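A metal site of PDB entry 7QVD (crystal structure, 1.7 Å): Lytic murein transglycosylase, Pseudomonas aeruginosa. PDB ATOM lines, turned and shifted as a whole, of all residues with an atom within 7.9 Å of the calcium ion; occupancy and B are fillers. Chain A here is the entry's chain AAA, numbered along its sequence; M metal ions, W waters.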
ATOM      1  N   ASP A 147       0.467 -18.360 -18.854  1.00  0.00           N
ATOM      2  CA  ASP A 147       1.013 -17.304 -19.751  1.00  0.00           C
ATOM      3  C   ASP A 147       0.313 -17.451 -21.108  1.00  0.00           C
ATOM      4  O   ASP A 147      -0.158 -16.434 -21.671  1.00  0.00           O
ATOM      5  CB  ASP A 147       2.536 -17.395 -19.829  1.00  0.00           C
ATOM      6  CG  ASP A 147       3.245 -16.702 -18.663  1.00  0.00           C
ATOM      7  OD1 ASP A 147       2.564 -15.989 -17.890  1.00  0.00           O
ATOM      8  OD2 ASP A 147       4.487 -16.885 -18.545  1.00  0.00           O
ATOM      9  N   VAL A 176       8.048 -10.631 -21.081  1.00  0.00           N
ATOM     10  CA  VAL A 176       7.779  -9.772 -19.897  1.00  0.00           C
ATOM     11  C   VAL A 176       6.282  -9.547 -19.708  1.00  0.00           C
ATOM     12  O   VAL A 176       5.493  -9.578 -20.684  1.00  0.00           O
ATOM     13  CB  VAL A 176       8.534  -8.444 -19.994  1.00  0.00           C
ATOM     14  CG1 VAL A 176      10.007  -8.687 -20.278  1.00  0.00           C
ATOM     15  CG2 VAL A 176       7.937  -7.475 -21.016  1.00  0.00           C
ATOM     16  N   ASP A 177       5.927  -9.306 -18.444  1.00  0.00           N
ATOM     17  CA  ASP A 177       4.571  -8.871 -18.053  1.00  0.00           C
ATOM     18  C   ASP A 177       4.581  -7.350 -17.968  1.00  0.00           C
ATOM     19  O   ASP A 177       4.855  -6.821 -16.883  1.00  0.00           O
ATOM     20  CB  ASP A 177       4.159  -9.509 -16.733  1.00  0.00           C
ATOM     21  CG  ASP A 177       2.822  -8.975 -16.240  1.00  0.00           C
ATOM     22  OD1 ASP A 177       2.068  -8.429 -17.047  1.00  0.00           O
ATOM     23  OD2 ASP A 177       2.575  -9.094 -15.023  1.00  0.00           O
ATOM     24  N   PHE A 178       4.365  -6.658 -19.080  1.00  0.00           N
ATOM     25  CA  PHE A 178       4.591  -5.195 -19.121  1.00  0.00           C
ATOM     26  C   PHE A 178       3.511  -4.497 -18.281  1.00  0.00           C
ATOM     27  O   PHE A 178       3.784  -3.480 -17.607  1.00  0.00           O
ATOM     28  CB  PHE A 178       4.590  -4.694 -20.559  1.00  0.00           C
ATOM     29  CG  PHE A 178       5.137  -3.306 -20.646  1.00  0.00           C
ATOM     30  CD1 PHE A 178       4.308  -2.204 -20.550  1.00  0.00           C
ATOM     31  CD2 PHE A 178       6.506  -3.111 -20.760  1.00  0.00           C
ATOM     32  CE1 PHE A 178       4.843  -0.928 -20.571  1.00  0.00           C
ATOM     33  CE2 PHE A 178       7.035  -1.830 -20.775  1.00  0.00           C
ATOM     34  CZ  PHE A 178       6.199  -0.741 -20.705  1.00  0.00           C
ATOM     35  N   ASP A 179       2.270  -4.987 -18.401  1.00  0.00           N
ATOM     36  CA  ASP A 179       1.082  -4.307 -17.846  1.00  0.00           C
ATOM     37  C   ASP A 179       0.877  -4.718 -16.374  1.00  0.00           C
ATOM     38  O   ASP A 179       0.042  -4.090 -15.733  1.00  0.00           O
ATOM     39  CB  ASP A 179      -0.168  -4.512 -18.719  1.00  0.00           C
ATOM     40  CG  ASP A 179      -0.478  -5.960 -19.121  1.00  0.00           C
ATOM     41  OD1 ASP A 179       0.053  -6.918 -18.451  1.00  0.00           O
ATOM     42  OD2 ASP A 179      -1.219  -6.126 -20.162  1.00  0.00           O
ATOM     43  N   GLY A 180       1.592  -5.736 -15.886  1.00  0.00           N
ATOM     44  CA  GLY A 180       1.668  -6.040 -14.442  1.00  0.00           C
ATOM     45  C   GLY A 180       0.456  -6.837 -13.942  1.00  0.00           C
ATOM     46  O   GLY A 180       0.205  -6.809 -12.696  1.00  0.00           O
ATOM     47  N   ASP A 181      -0.250  -7.562 -14.822  1.00  0.00           N
ATOM     48  CA  ASP A 181      -1.441  -8.362 -14.425  1.00  0.00           C
ATOM     49  C   ASP A 181      -1.037  -9.776 -14.005  1.00  0.00           C
ATOM     50  O   ASP A 181      -1.953 -10.604 -13.803  1.00  0.00           O
ATOM     51  CB  ASP A 181      -2.483  -8.411 -15.545  1.00  0.00           C
ATOM     52  CG  ASP A 181      -2.009  -9.187 -16.767  1.00  0.00           C
ATOM     53  OD1 ASP A 181      -0.771  -9.444 -16.865  1.00  0.00           O
ATOM     54  OD2 ASP A 181      -2.873  -9.566 -17.599  1.00  0.00           O
ATOM     55  N   GLY A 182       0.266 -10.074 -13.927  1.00  0.00           N
ATOM     56  CA  GLY A 182       0.817 -11.357 -13.463  1.00  0.00           C
ATOM     57  C   GLY A 182       0.921 -12.353 -14.609  1.00  0.00           C
ATOM     58  O   GLY A 182       1.299 -13.521 -14.378  1.00  0.00           O
ATOM     59  N   ARG A 183       0.595 -11.917 -15.816  1.00  0.00           N
ATOM     60  CA  ARG A 183       0.568 -12.806 -17.001  1.00  0.00           C
ATOM     61  C   ARG A 183       1.514 -12.283 -18.071  1.00  0.00           C
ATOM     62  O   ARG A 183       1.483 -11.075 -18.313  1.00  0.00           O
ATOM     63  CB  ARG A 183      -0.854 -12.847 -17.540  1.00  0.00           C
ATOM     64  CG  ARG A 183      -1.044 -13.830 -18.660  1.00  0.00           C
ATOM     65  CD  ARG A 183      -2.510 -13.992 -18.999  1.00  0.00           C
ATOM     66  NE  ARG A 183      -2.572 -14.809 -20.196  1.00  0.00           N
ATOM     67  CZ  ARG A 183      -3.632 -14.894 -20.998  1.00  0.00           C
ATOM     68  NH1 ARG A 183      -4.730 -14.218 -20.715  1.00  0.00           N
ATOM     69  NH2 ARG A 183      -3.571 -15.647 -22.086  1.00  0.00           N
ATOM     70  N   ARG A 184       2.335 -13.151 -18.666  1.00  0.00           N
ATOM     71  CA  ARG A 184       3.193 -12.802 -19.833  1.00  0.00           C
ATOM     72  C   ARG A 184       2.455 -13.318 -21.074  1.00  0.00           C
ATOM     73  O   ARG A 184       2.630 -14.493 -21.412  1.00  0.00           O
ATOM     74  CB  ARG A 184       4.592 -13.417 -19.709  1.00  0.00           C
ATOM     75  CG  ARG A 184       5.314 -12.974 -18.453  1.00  0.00           C
ATOM     76  CD  ARG A 184       6.738 -13.471 -18.389  1.00  0.00           C
ATOM     77  NE  ARG A 184       6.816 -14.920 -18.387  1.00  0.00           N
ATOM     78  CZ  ARG A 184       7.887 -15.639 -18.717  1.00  0.00           C
ATOM     79  NH1 ARG A 184       9.006 -15.042 -19.085  1.00  0.00           N
ATOM     80  NH2 ARG A 184       7.829 -16.956 -18.672  1.00  0.00           N
ATOM     81  N   ASP A 185       1.640 -12.468 -21.675  1.00  0.00           N
ATOM     82  CA  ASP A 185       0.645 -12.840 -22.708  1.00  0.00           C
ATOM     83  C   ASP A 185       1.051 -12.200 -24.035  1.00  0.00           C
ATOM     84  O   ASP A 185       0.607 -11.093 -24.300  1.00  0.00           O
ATOM     85  CB  ASP A 185      -0.768 -12.400 -22.307  1.00  0.00           C
ATOM     86  CG  ASP A 185      -1.796 -12.663 -23.395  1.00  0.00           C
ATOM     87  OD1 ASP A 185      -1.459 -13.416 -24.351  1.00  0.00           O
ATOM     88  OD2 ASP A 185      -2.900 -12.112 -23.290  1.00  0.00           O
ATOM     89  N   LEU A 186       1.857 -12.883 -24.837  1.00  0.00           N
ATOM     90  CA  LEU A 186       2.383 -12.325 -26.107  1.00  0.00           C
ATOM     91  C   LEU A 186       1.420 -12.649 -27.260  1.00  0.00           C
ATOM     92  O   LEU A 186       1.768 -12.381 -28.440  1.00  0.00           O
ATOM     93  CB  LEU A 186       3.785 -12.867 -26.343  1.00  0.00           C
ATOM     94  CG  LEU A 186       4.922 -12.173 -25.576  1.00  0.00           C
ATOM     95  CD1 LEU A 186       4.612 -11.937 -24.105  1.00  0.00           C
ATOM     96  CD2 LEU A 186       6.197 -12.980 -25.732  1.00  0.00           C
ATOM     97  N   SER A 189      -1.876  -9.498 -25.376  1.00  0.00           N
ATOM     98  CA  SER A 189      -1.488  -8.238 -24.698  1.00  0.00           C
ATOM     99  C   SER A 189      -0.499  -7.475 -25.579  1.00  0.00           C
ATOM    100  O   SER A 189       0.658  -7.898 -25.669  1.00  0.00           O
ATOM    101  CB  SER A 189      -0.895  -8.498 -23.328  1.00  0.00           C
ATOM    102  OG  SER A 189      -0.383  -7.293 -22.779  1.00  0.00           O
ATOM    103  N   PRO A 191       0.795  -4.533 -24.738  1.00  0.00           N
ATOM    104  CA  PRO A 191       1.861  -4.130 -23.838  1.00  0.00           C
ATOM    105  C   PRO A 191       2.898  -5.241 -23.623  1.00  0.00           C
ATOM    106  O   PRO A 191       4.075  -4.977 -23.751  1.00  0.00           O
ATOM    107  CB  PRO A 191       1.145  -3.761 -22.529  1.00  0.00           C
ATOM    108  CG  PRO A 191      -0.228  -3.302 -23.022  1.00  0.00           C
ATOM    109  CD  PRO A 191      -0.537  -4.224 -24.181  1.00  0.00           C
ATOM    110  N   ASP A 192       2.466  -6.453 -23.296  1.00  0.00           N
ATOM    111  CA  ASP A 192       3.430  -7.556 -23.055  1.00  0.00           C
ATOM    112  C   ASP A 192       4.228  -7.816 -24.341  1.00  0.00           C
ATOM    113  O   ASP A 192       5.450  -8.044 -24.263  1.00  0.00           O
ATOM    114  CB  ASP A 192       2.765  -8.847 -22.596  1.00  0.00           C
ATOM    115  CG  ASP A 192       2.040  -8.764 -21.260  1.00  0.00           C
ATOM    116  OD1 ASP A 192       2.225  -7.769 -20.518  1.00  0.00           O
ATOM    117  OD2 ASP A 192       1.335  -9.739 -20.952  1.00  0.00           O
ATOM    118  N   ALA A 193       3.565  -7.816 -25.498  1.00  0.00           N
ATOM    119  CA  ALA A 193       4.229  -8.073 -26.803  1.00  0.00           C
ATOM    120  C   ALA A 193       5.300  -7.026 -27.087  1.00  0.00           C
ATOM    121  O   ALA A 193       6.421  -7.389 -27.452  1.00  0.00           O
ATOM    122  CB  ALA A 193       3.226  -8.090 -27.932  1.00  0.00           C
HETATM  123 CA    CA M   1       0.588  -9.003 -18.779  1.00  0.00          CA
HETATM  124  O   HOH W   1      -1.337  -9.648 -19.722  1.00  0.00           O
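The calcium ion is bound by the side-chain carboxylate (OD1) of Asp 179 (2.2 Å), water W1 (2.2 Å), the backbone carbonyl oxygen (O) of Arg 183 (2.3 Å), the side-chain carboxylate (OD1) of Asp 177 (2.3 Å), the side-chain carboxylate (OD1) of Asp 181 (2.4 Å), the side-chain carboxylate (OD2) of Asp 192 (2.4 Å) and the side-chain carboxylate (OD1) of Asp 192 (2.7 Å).
Of the 16 residues printed, 5 come within 4 Å of the calcium ion.
Along chain A the residues within 4 Å of the calcium ion span positions 177 to 192.
The side-chain carboxylate (OD2) of Asp 179 sits at hydrogen-bond distance from the side-chain hydroxyl (OG) of Ser 189 (3.0 Å).
N of Asp 185 lies close to OD2 of Asp 192 (2.8 Å).
The guanidinium group of Arg 183 lies within hydrogen-bond range of the backbone carbonyl oxygen of Asp 147.
The backbone NH (N) of Asp 192 is in hydrogen-bond range of the side-chain hydroxyl (OG) of Ser 189 (3.0 Å).
N of Gly 182 sits at hydrogen-bond distance from OD2 of Asp 177 (2.7 Å).
The guanidinium group of Arg 183 lies within salt-bridge range of the side-chain carboxylate of Asp 185 (3.8 Å).
The side-chain carboxylate (OD1) of Asp 192 sits close to the backbone NH (N) of Phe 178.
N of Gly 180 lies close to OD1 of Asp 177 (3.0 Å).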
